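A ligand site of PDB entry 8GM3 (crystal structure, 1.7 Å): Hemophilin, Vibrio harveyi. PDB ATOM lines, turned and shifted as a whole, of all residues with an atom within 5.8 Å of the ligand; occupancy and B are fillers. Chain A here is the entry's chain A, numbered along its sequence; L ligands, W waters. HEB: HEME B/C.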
ATOM      1  N   ARG A  12     -19.782   7.789 -18.099  1.00  0.00           N
ATOM      2  CA  ARG A  12     -19.196   6.483 -17.827  1.00  0.00           C
ATOM      3  C   ARG A  12     -17.736   6.676 -17.460  1.00  0.00           C
ATOM      4  O   ARG A  12     -17.122   7.708 -17.750  1.00  0.00           O
ATOM      5  CB  ARG A  12     -19.319   5.543 -19.035  1.00  0.00           C
ATOM      6  CG  ARG A  12     -20.728   5.139 -19.357  1.00  0.00           C
ATOM      7  CD  ARG A  12     -21.315   4.368 -18.213  1.00  0.00           C
ATOM      8  NE  ARG A  12     -22.632   3.800 -18.489  1.00  0.00           N
ATOM      9  CZ  ARG A  12     -23.779   4.451 -18.287  1.00  0.00           C
ATOM     10  NH1 ARG A  12     -23.759   5.705 -17.853  1.00  0.00           N
ATOM     11  NH2 ARG A  12     -24.937   3.863 -18.538  1.00  0.00           N
ATOM     12  N   VAL A  19     -18.821  -4.441  -8.429  1.00  0.00           N
ATOM     13  CA  VAL A  19     -20.144  -4.954  -8.106  1.00  0.00           C
ATOM     14  C   VAL A  19     -20.072  -6.472  -8.086  1.00  0.00           C
ATOM     15  O   VAL A  19     -19.604  -7.094  -9.041  1.00  0.00           O
ATOM     16  CB  VAL A  19     -21.171  -4.496  -9.148  1.00  0.00           C
ATOM     17  CG1 VAL A  19     -22.489  -5.243  -8.958  1.00  0.00           C
ATOM     18  CG2 VAL A  19     -21.369  -2.983  -9.093  1.00  0.00           C
ATOM     19  N   VAL A  21     -22.638  -9.522  -7.999  1.00  0.00           N
ATOM     20  CA  VAL A  21     -23.995 -10.063  -8.058  1.00  0.00           C
ATOM     21  C   VAL A  21     -23.865 -11.495  -8.576  1.00  0.00           C
ATOM     22  O   VAL A  21     -23.512 -11.694  -9.737  1.00  0.00           O
ATOM     23  CB  VAL A  21     -24.914  -9.217  -8.956  1.00  0.00           C
ATOM     24  CG1 VAL A  21     -26.238  -9.939  -9.185  1.00  0.00           C
ATOM     25  CG2 VAL A  21     -25.156  -7.869  -8.300  1.00  0.00           C
ATOM     26  N   ILE A  24     -23.459 -12.921 -12.503  1.00  0.00           N
ATOM     27  CA  ILE A  24     -23.554 -11.876 -13.518  1.00  0.00           C
ATOM     28  C   ILE A  24     -22.441 -10.858 -13.365  1.00  0.00           C
ATOM     29  O   ILE A  24     -21.638 -10.648 -14.293  1.00  0.00           O
ATOM     30  CB  ILE A  24     -24.938 -11.209 -13.498  1.00  0.00           C
ATOM     31  CG1 ILE A  24     -24.944  -9.949 -14.352  1.00  0.00           C
ATOM     32  CG2 ILE A  24     -25.324 -10.874 -12.085  1.00  0.00           C
ATOM     33  CD1 ILE A  24     -24.507 -10.173 -15.808  1.00  0.00           C
ATOM     34  N   HIS A  25     -22.360 -10.219 -12.195  1.00  0.00           N
ATOM     35  CA  HIS A  25     -21.365  -9.207 -11.898  1.00  0.00           C
ATOM     36  C   HIS A  25     -20.346  -9.738 -10.900  1.00  0.00           C
ATOM     37  O   HIS A  25     -20.716 -10.254  -9.842  1.00  0.00           O
ATOM     38  CB  HIS A  25     -22.044  -7.949 -11.336  1.00  0.00           C
ATOM     39  CG  HIS A  25     -22.927  -7.272 -12.324  1.00  0.00           C
ATOM     40  ND1 HIS A  25     -22.677  -7.277 -13.677  1.00  0.00           N
ATOM     41  CD2 HIS A  25     -24.070  -6.560 -12.159  1.00  0.00           C
ATOM     42  CE1 HIS A  25     -23.629  -6.596 -14.298  1.00  0.00           C
ATOM     43  NE2 HIS A  25     -24.484  -6.161 -13.405  1.00  0.00           N
ATOM     44  N   ILE A  32     -16.421  -1.202 -16.201  1.00  0.00           N
ATOM     45  CA  ILE A  32     -16.956   0.096 -16.606  1.00  0.00           C
ATOM     46  C   ILE A  32     -18.224   0.356 -15.805  1.00  0.00           C
ATOM     47  O   ILE A  32     -18.912  -0.579 -15.417  1.00  0.00           O
ATOM     48  CB  ILE A  32     -17.235   0.132 -18.125  1.00  0.00           C
ATOM     49  CG1 ILE A  32     -17.620   1.546 -18.572  1.00  0.00           C
ATOM     50  CG2 ILE A  32     -18.348  -0.864 -18.485  1.00  0.00           C
ATOM     51  CD1 ILE A  32     -17.647   1.685 -20.100  1.00  0.00           C
ATOM     52  N   GLY A  33     -18.552   1.621 -15.614  1.00  0.00           N
ATOM     53  CA  GLY A  33     -19.753   1.917 -14.835  1.00  0.00           C
ATOM     54  C   GLY A  33     -20.147   3.375 -14.906  1.00  0.00           C
ATOM     55  O   GLY A  33     -19.402   4.235 -15.397  1.00  0.00           O
ATOM     56  N   LYS A  34     -21.337   3.645 -14.400  1.00  0.00           N
ATOM     57  CA  LYS A  34     -21.862   5.008 -14.364  1.00  0.00           C
ATOM     58  C   LYS A  34     -20.930   5.894 -13.557  1.00  0.00           C
ATOM     59  O   LYS A  34     -20.449   5.505 -12.478  1.00  0.00           O
ATOM     60  CB  LYS A  34     -23.265   4.977 -13.753  1.00  0.00           C
ATOM     61  CG  LYS A  34     -23.973   6.296 -13.606  1.00  0.00           C
ATOM     62  CD  LYS A  34     -25.475   6.060 -13.379  1.00  0.00           C
ATOM     63  CE  LYS A  34     -26.106   5.325 -14.564  1.00  0.00           C
ATOM     64  NZ  LYS A  34     -27.547   5.654 -14.759  1.00  0.00           N
ATOM     65  N   GLY A  36     -20.241   8.349 -10.872  1.00  0.00           N
ATOM     66  CA  GLY A  36     -20.981   8.425  -9.644  1.00  0.00           C
ATOM     67  C   GLY A  36     -21.529   7.100  -9.156  1.00  0.00           C
ATOM     68  O   GLY A  36     -22.168   7.066  -8.103  1.00  0.00           O
ATOM     69  N   GLY A  37     -21.294   6.018  -9.899  1.00  0.00           N
ATOM     70  CA  GLY A  37     -21.804   4.710  -9.513  1.00  0.00           C
ATOM     71  C   GLY A  37     -20.707   3.686  -9.412  1.00  0.00           C
ATOM     72  O   GLY A  37     -19.531   4.041  -9.321  1.00  0.00           O
ATOM     73  N   LYS A  38     -21.053   2.400  -9.446  1.00  0.00           N
ATOM     74  CA  LYS A  38     -20.073   1.338  -9.312  1.00  0.00           C
ATOM     75  C   LYS A  38     -19.858   0.635 -10.653  1.00  0.00           C
ATOM     76  O   LYS A  38     -20.773   0.526 -11.472  1.00  0.00           O
ATOM     77  CB  LYS A  38     -20.498   0.333  -8.252  1.00  0.00           C
ATOM     78  CG  LYS A  38     -20.675   0.917  -6.874  1.00  0.00           C
ATOM     79  CD  LYS A  38     -19.324   1.276  -6.252  1.00  0.00           C
ATOM     80  CE  LYS A  38     -19.464   1.590  -4.752  1.00  0.00           C
ATOM     81  NZ  LYS A  38     -18.141   1.631  -4.077  1.00  0.00           N
ATOM     82  N   ARG A  39     -18.640   0.140 -10.851  1.00  0.00           N
ATOM     83  CA  ARG A  39     -18.243  -0.491 -12.102  1.00  0.00           C
ATOM     84  C   ARG A  39     -18.577  -1.972 -12.107  1.00  0.00           C
ATOM     85  O   ARG A  39     -18.394  -2.667 -11.116  1.00  0.00           O
ATOM     86  CB  ARG A  39     -16.749  -0.290 -12.335  1.00  0.00           C
ATOM     87  CG  ARG A  39     -16.352   1.169 -12.459  1.00  0.00           C
ATOM     88  CD  ARG A  39     -14.901   1.338 -12.913  1.00  0.00           C
ATOM     89  NE  ARG A  39     -13.970   0.951 -11.852  1.00  0.00           N
ATOM     90  CZ  ARG A  39     -13.565   1.756 -10.883  1.00  0.00           C
ATOM     91  NH1 ARG A  39     -13.973   3.023 -10.827  1.00  0.00           N
ATOM     92  NH2 ARG A  39     -12.717   1.309  -9.976  1.00  0.00           N
ATOM     93  N   VAL A  40     -19.071  -2.458 -13.248  1.00  0.00           N
ATOM     94  CA  VAL A  40     -19.283  -3.882 -13.467  1.00  0.00           C
ATOM     95  C   VAL A  40     -18.258  -4.355 -14.487  1.00  0.00           C
ATOM     96  O   VAL A  40     -17.634  -3.568 -15.205  1.00  0.00           O
ATOM     97  CB  VAL A  40     -20.723  -4.187 -13.914  1.00  0.00           C
ATOM     98  CG1 VAL A  40     -21.737  -3.650 -12.894  1.00  0.00           C
ATOM     99  CG2 VAL A  40     -20.982  -3.645 -15.318  1.00  0.00           C
ATOM    100  N   LEU A  45     -20.558  -9.205 -19.044  1.00  0.00           N
ATOM    101  CA  LEU A  45     -21.398  -8.690 -20.117  1.00  0.00           C
ATOM    102  C   LEU A  45     -21.241  -9.520 -21.398  1.00  0.00           C
ATOM    103  O   LEU A  45     -22.222  -9.761 -22.105  1.00  0.00           O
ATOM    104  CB  LEU A  45     -21.052  -7.227 -20.406  1.00  0.00           C
ATOM    105  CG  LEU A  45     -21.302  -6.214 -19.292  1.00  0.00           C
ATOM    106  CD1 LEU A  45     -21.079  -4.801 -19.818  1.00  0.00           C
ATOM    107  CD2 LEU A  45     -22.719  -6.357 -18.754  1.00  0.00           C
ATOM    108  N   ILE A  49     -27.115 -12.338 -21.451  1.00  0.00           N
ATOM    109  CA  ILE A  49     -28.436 -12.329 -22.054  1.00  0.00           C
ATOM    110  C   ILE A  49     -28.706 -11.039 -22.814  1.00  0.00           C
ATOM    111  O   ILE A  49     -29.555 -11.020 -23.710  1.00  0.00           O
ATOM    112  CB  ILE A  49     -29.516 -12.572 -20.978  1.00  0.00           C
ATOM    113  CG1 ILE A  49     -29.461 -11.465 -19.926  1.00  0.00           C
ATOM    114  CG2 ILE A  49     -29.354 -13.938 -20.352  1.00  0.00           C
ATOM    115  CD1 ILE A  49     -30.651 -11.449 -18.984  1.00  0.00           C
ATOM    116  N   PHE A  50     -28.033  -9.941 -22.476  1.00  0.00           N
ATOM    117  CA  PHE A  50     -28.190  -8.693 -23.200  1.00  0.00           C
ATOM    118  C   PHE A  50     -27.115  -8.493 -24.271  1.00  0.00           C
ATOM    119  O   PHE A  50     -27.041  -7.418 -24.877  1.00  0.00           O
ATOM    120  CB  PHE A  50     -28.174  -7.505 -22.224  1.00  0.00           C
ATOM    121  CG  PHE A  50     -29.438  -7.343 -21.443  1.00  0.00           C
ATOM    122  CD1 PHE A  50     -29.727  -8.161 -20.368  1.00  0.00           C
ATOM    123  CD2 PHE A  50     -30.341  -6.353 -21.780  1.00  0.00           C
ATOM    124  CE1 PHE A  50     -30.893  -8.014 -19.654  1.00  0.00           C
ATOM    125  CE2 PHE A  50     -31.511  -6.193 -21.056  1.00  0.00           C
ATOM    126  CZ  PHE A  50     -31.778  -7.024 -19.995  1.00  0.00           C
ATOM    127  N   SER A  60     -23.776  -4.831 -25.909  1.00  0.00           N
ATOM    128  CA  SER A  60     -24.642  -5.188 -24.793  1.00  0.00           C
ATOM    129  C   SER A  60     -25.439  -3.989 -24.323  1.00  0.00           C
ATOM    130  O   SER A  60     -24.892  -2.890 -24.174  1.00  0.00           O
ATOM    131  CB  SER A  60     -23.864  -5.756 -23.621  1.00  0.00           C
ATOM    132  OG  SER A  60     -24.783  -6.103 -22.594  1.00  0.00           O
ATOM    133  N   GLY A  61     -26.722  -4.218 -24.064  1.00  0.00           N
ATOM    134  CA  GLY A  61     -27.532  -3.281 -23.341  1.00  0.00           C
ATOM    135  C   GLY A  61     -27.345  -3.455 -21.844  1.00  0.00           C
ATOM    136  O   GLY A  61     -26.512  -4.238 -21.374  1.00  0.00           O
ATOM    137  N   SER A  62     -28.112  -2.687 -21.086  1.00  0.00           N
ATOM    138  CA  SER A  62     -28.134  -2.768 -19.629  1.00  0.00           C
ATOM    139  C   SER A  62     -29.463  -3.353 -19.162  1.00  0.00           C
ATOM    140  O   SER A  62     -30.524  -2.975 -19.666  1.00  0.00           O
ATOM    141  CB  SER A  62     -27.945  -1.386 -19.017  1.00  0.00           C
ATOM    142  OG  SER A  62     -27.934  -1.478 -17.601  1.00  0.00           O
ATOM    143  N   LYS A  63     -29.415  -4.258 -18.177  1.00  0.00           N
ATOM    144  CA  LYS A  63     -30.650  -4.686 -17.531  1.00  0.00           C
ATOM    145  C   LYS A  63     -31.402  -3.500 -16.954  1.00  0.00           C
ATOM    146  O   LYS A  63     -32.642  -3.484 -16.915  1.00  0.00           O
ATOM    147  CB  LYS A  63     -30.349  -5.694 -16.431  1.00  0.00           C
ATOM    148  CG  LYS A  63     -31.559  -6.358 -15.842  1.00  0.00           C
ATOM    149  CD  LYS A  63     -31.239  -6.981 -14.485  1.00  0.00           C
ATOM    150  CE  LYS A  63     -32.318  -7.980 -14.048  1.00  0.00           C
ATOM    151  NZ  LYS A  63     -33.664  -7.352 -13.994  1.00  0.00           N
ATOM    152  N   HIS A  64     -30.673  -2.468 -16.543  1.00  0.00           N
ATOM    153  CA  HIS A  64     -31.220  -1.479 -15.619  1.00  0.00           C
ATOM    154  C   HIS A  64     -31.889  -0.311 -16.318  1.00  0.00           C
ATOM    155  O   HIS A  64     -32.908   0.193 -15.832  1.00  0.00           O
ATOM    156  CB  HIS A  64     -30.101  -1.030 -14.686  1.00  0.00           C
ATOM    157  CG  HIS A  64     -29.431  -2.200 -14.042  1.00  0.00           C
ATOM    158  ND1 HIS A  64     -30.123  -3.093 -13.256  1.00  0.00           N
ATOM    159  CD2 HIS A  64     -28.173  -2.691 -14.155  1.00  0.00           C
ATOM    160  CE1 HIS A  64     -29.317  -4.058 -12.872  1.00  0.00           C
ATOM    161  NE2 HIS A  64     -28.120  -3.829 -13.390  1.00  0.00           N
ATOM    162  N   PHE A  65     -31.338   0.125 -17.446  1.00  0.00           N
ATOM    163  CA  PHE A  65     -31.883   1.272 -18.168  1.00  0.00           C
ATOM    164  C   PHE A  65     -31.873   0.921 -19.641  1.00  0.00           C
ATOM    165  O   PHE A  65     -30.880   0.391 -20.142  1.00  0.00           O
ATOM    166  CB  PHE A  65     -31.061   2.535 -17.933  1.00  0.00           C
ATOM    167  CG  PHE A  65     -31.021   2.969 -16.506  1.00  0.00           C
ATOM    168  CD1 PHE A  65     -30.022   2.512 -15.663  1.00  0.00           C
ATOM    169  CD2 PHE A  65     -31.986   3.819 -16.005  1.00  0.00           C
ATOM    170  CE1 PHE A  65     -29.992   2.908 -14.343  1.00  0.00           C
ATOM    171  CE2 PHE A  65     -31.952   4.215 -14.694  1.00  0.00           C
ATOM    172  CZ  PHE A  65     -30.968   3.767 -13.868  1.00  0.00           C
ATOM    173  N   ASN A  68     -29.440   2.445 -24.096  1.00  0.00           N
ATOM    174  CA  ASN A  68     -28.020   2.783 -24.139  1.00  0.00           C
ATOM    175  C   ASN A  68     -27.258   1.471 -24.284  1.00  0.00           C
ATOM    176  O   ASN A  68     -27.741   0.423 -23.870  1.00  0.00           O
ATOM    177  CB  ASN A  68     -27.564   3.549 -22.887  1.00  0.00           C
ATOM    178  CG  ASN A  68     -27.694   2.735 -21.609  1.00  0.00           C
ATOM    179  OD1 ASN A  68     -26.700   2.379 -20.967  1.00  0.00           O
ATOM    180  ND2 ASN A  68     -28.929   2.450 -21.224  1.00  0.00           N
ATOM    181  N   TYR A  70     -23.262  -0.698 -25.001  1.00  0.00           N
ATOM    182  CA  TYR A  70     -21.812  -0.836 -25.058  1.00  0.00           C
ATOM    183  C   TYR A  70     -21.470  -1.754 -26.210  1.00  0.00           C
ATOM    184  O   TYR A  70     -21.995  -2.859 -26.305  1.00  0.00           O
ATOM    185  CB  TYR A  70     -21.263  -1.442 -23.762  1.00  0.00           C
ATOM    186  CG  TYR A  70     -21.648  -0.751 -22.477  1.00  0.00           C
ATOM    187  CD1 TYR A  70     -22.888  -0.996 -21.881  1.00  0.00           C
ATOM    188  CD2 TYR A  70     -20.769   0.088 -21.820  1.00  0.00           C
ATOM    189  CE1 TYR A  70     -23.242  -0.397 -20.679  1.00  0.00           C
ATOM    190  CE2 TYR A  70     -21.119   0.702 -20.626  1.00  0.00           C
ATOM    191  CZ  TYR A  70     -22.346   0.446 -20.058  1.00  0.00           C
ATOM    192  OH  TYR A  70     -22.681   1.055 -18.880  1.00  0.00           O
ATOM    193  N   TRP A  85     -19.465   3.489 -25.587  1.00  0.00           N
ATOM    194  CA  TRP A  85     -20.800   3.477 -25.021  1.00  0.00           C
ATOM    195  C   TRP A  85     -21.540   4.694 -25.570  1.00  0.00           C
ATOM    196  O   TRP A  85     -20.926   5.707 -25.883  1.00  0.00           O
ATOM    197  CB  TRP A  85     -20.759   3.513 -23.479  1.00  0.00           C
ATOM    198  CG  TRP A  85     -22.075   3.738 -22.803  1.00  0.00           C
ATOM    199  CD1 TRP A  85     -22.935   2.778 -22.363  1.00  0.00           C
ATOM    200  CD2 TRP A  85     -22.675   4.998 -22.470  1.00  0.00           C
ATOM    201  NE1 TRP A  85     -24.043   3.366 -21.787  1.00  0.00           N
ATOM    202  CE2 TRP A  85     -23.895   4.727 -21.835  1.00  0.00           C
ATOM    203  CE3 TRP A  85     -22.284   6.328 -22.653  1.00  0.00           C
ATOM    204  CZ2 TRP A  85     -24.749   5.738 -21.388  1.00  0.00           C
ATOM    205  CZ3 TRP A  85     -23.137   7.339 -22.206  1.00  0.00           C
ATOM    206  CH2 TRP A  85     -24.351   7.032 -21.572  1.00  0.00           C
HETATM  207 FE   HEB L   1     -26.324  -4.960 -13.448  1.00  0.00          FE
HETATM  208  CHA HEB L   1     -24.576  -2.096 -13.096  1.00  0.00           C
HETATM  209  CHB HEB L   1     -26.806  -5.070  -9.976  1.00  0.00           C
HETATM  210  CHC HEB L   1     -28.158  -7.797 -13.725  1.00  0.00           C
HETATM  211  CHD HEB L   1     -25.734  -4.952 -16.793  1.00  0.00           C
HETATM  212  NA  HEB L   1     -25.807  -3.842 -11.846  1.00  0.00           N
HETATM  213  C1A HEB L   1     -25.062  -2.684 -11.943  1.00  0.00           C
HETATM  214  C2A HEB L   1     -24.865  -2.143 -10.610  1.00  0.00           C
HETATM  215  C3A HEB L   1     -25.465  -2.975  -9.743  1.00  0.00           C
HETATM  216  C4A HEB L   1     -26.074  -4.042 -10.500  1.00  0.00           C
HETATM  217  CMA HEB L   1     -25.534  -2.821  -8.217  1.00  0.00           C
HETATM  218  CAA HEB L   1     -24.077  -0.854 -10.278  1.00  0.00           C
HETATM  219  CBA HEB L   1     -25.035   0.321 -10.412  1.00  0.00           C
HETATM  220  CGA HEB L   1     -24.411   1.634 -10.019  1.00  0.00           C
HETATM  221  O1A HEB L   1     -24.523   2.605 -10.817  1.00  0.00           O
HETATM  222  O2A HEB L   1     -23.806   1.760  -8.920  1.00  0.00           O
HETATM  223  NB  HEB L   1     -27.264  -6.212 -12.082  1.00  0.00           N
HETATM  224  C1B HEB L   1     -27.420  -6.031 -10.724  1.00  0.00           C
HETATM  225  C2B HEB L   1     -28.359  -7.030 -10.235  1.00  0.00           C
HETATM  226  C3B HEB L   1     -28.727  -7.785 -11.282  1.00  0.00           C
HETATM  227  C4B HEB L   1     -28.044  -7.290 -12.455  1.00  0.00           C
HETATM  228  CMB HEB L   1     -28.782  -7.150  -8.753  1.00  0.00           C
HETATM  229  CAB HEB L   1     -29.693  -9.010 -11.324  1.00  0.00           C
HETATM  230  CBB HEB L   1     -30.341  -9.446 -10.239  1.00  0.00           C
HETATM  231  NC  HEB L   1     -26.855  -6.108 -14.971  1.00  0.00           N
HETATM  232  C1C HEB L   1     -27.587  -7.282 -14.869  1.00  0.00           C
HETATM  233  C2C HEB L   1     -27.661  -7.899 -16.176  1.00  0.00           C
HETATM  234  C3C HEB L   1     -27.003  -7.119 -17.023  1.00  0.00           C
HETATM  235  C4C HEB L   1     -26.481  -5.984 -16.287  1.00  0.00           C
HETATM  236  CMC HEB L   1     -28.371  -9.218 -16.565  1.00  0.00           C
HETATM  237  CAC HEB L   1     -26.878  -7.470 -18.512  1.00  0.00           C
HETATM  238  CBC HEB L   1     -26.380  -6.592 -19.387  1.00  0.00           C
HETATM  239  ND  HEB L   1     -25.327  -3.764 -14.705  1.00  0.00           N
HETATM  240  C1D HEB L   1     -25.243  -3.901 -16.069  1.00  0.00           C
HETATM  241  C2D HEB L   1     -24.557  -2.742 -16.611  1.00  0.00           C
HETATM  242  C3D HEB L   1     -24.236  -1.941 -15.592  1.00  0.00           C
HETATM  243  C4D HEB L   1     -24.715  -2.572 -14.374  1.00  0.00           C
HETATM  244  CMD HEB L   1     -24.277  -2.491 -18.100  1.00  0.00           C
HETATM  245  CAD HEB L   1     -23.497  -0.584 -15.682  1.00  0.00           C
HETATM  246  CBD HEB L   1     -24.457   0.608 -15.650  1.00  0.00           C
HETATM  247  CGD HEB L   1     -25.431   0.600 -16.793  1.00  0.00           C
HETATM  248  O1D HEB L   1     -26.641   0.439 -16.516  1.00  0.00           O
HETATM  249  O2D HEB L   1     -25.031   0.744 -17.974  1.00  0.00           O
HETATM  250  O   HOH W   1     -27.036   0.808 -13.661  1.00  0.00           O
HETATM  251  O   HOH W   2     -25.013  -8.798 -21.730  1.00  0.00           O
HETATM  252  O   HOH W   3     -24.754   3.911  -7.705  1.00  0.00           O
HETATM  253  O   HOH W   4     -22.837   1.708 -12.674  1.00  0.00           O
HETATM  254  O   HOH W   5     -26.970   2.954 -11.958  1.00  0.00           O
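Residues that only touch the ligand: Val 19 (3.6 Å), Val 21 (3.7 Å), Ile 24 (3.8 Å), Lys 34 (3.98 Å), Gly 37 (3.6 Å), Val 40 (3.2 Å), Leu 45 (3.7 Å), Phe 50 (3.5 Å), Ser 60 (3.6 Å), Gly 61 (3.1 Å), Lys 63 (3.3 Å) and Asn 68 (3.8 Å). 18 residues have an atom within 4 Å of the ligand: Arg 12, Val 19, Val 21, Ile 24, His 25, Lys 34, Gly 37, Lys 38, Val 40, Leu 45, Phe 50, Ser 60, Gly 61, Ser 62, Lys 63, His 64, Asn 68 and Tyr 70. The nearest printed residue that does not touch the ligand is Ile 49 (4.003 Å).
The backbone NH of His 64 lies close to the side-chain hydroxyl of Ser 62 (3.1 Å). O of Arg 39 is in hydrogen-bond range of N of Val 19 (3.2 Å). O of Phe 50 lies close to OG of Ser 60 (3.5 Å). N of Gly 61 is in hydrogen-bond range of O of Phe 50 (3.3 Å). The side-chain amide nitrogen (ND2) of Asn 68 lies within hydrogen-bond range of the backbone carbonyl oxygen (O) of Phe 65 (3.0 Å). OH of Tyr 70 lies within hydrogen-bond range of NE of Arg 12 (2.8 Å). OD1 of Asn 68 lies within hydrogen-bond range of NE1 of Trp 85 (3.0 Å). O of Val 40 is in hydrogen-bond range of N of Ile 32, 2.8 Å away.
Water W4 lies within hydrogen-bond range of O1A of the ligand (2.7 Å), O of Lys 38 (2.7 Å) and N of Lys 34 (3.0 Å). Water W2 lies within hydrogen-bond range of OG of Ser 60 (2.8 Å), O of Leu 45 (3.0 Å) and N of Phe 50 (3.3 Å).
FE of the ligand is bound by NE2 of His 25 (2.2 Å). The side-chain hydroxyl of Tyr 70 lies within hydrogen-bond range of an oxygen (O2D) of the ligand (2.5 Å). NH2 of Arg 12 is in salt-bridge range of O2D of the ligand (3.2 Å). A ring nitrogen (NE2) of His 64 is bound to an iron atom (FE) of the ligand. An oxygen (O1D) of the ligand is in hydrogen-bond range of the side-chain hydroxyl (OG) of Ser 62, at 2.6 Å. The backbone NH of Lys 38 lies within hydrogen-bond range of an oxygen (O2A) of the ligand, 2.9 Å away.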
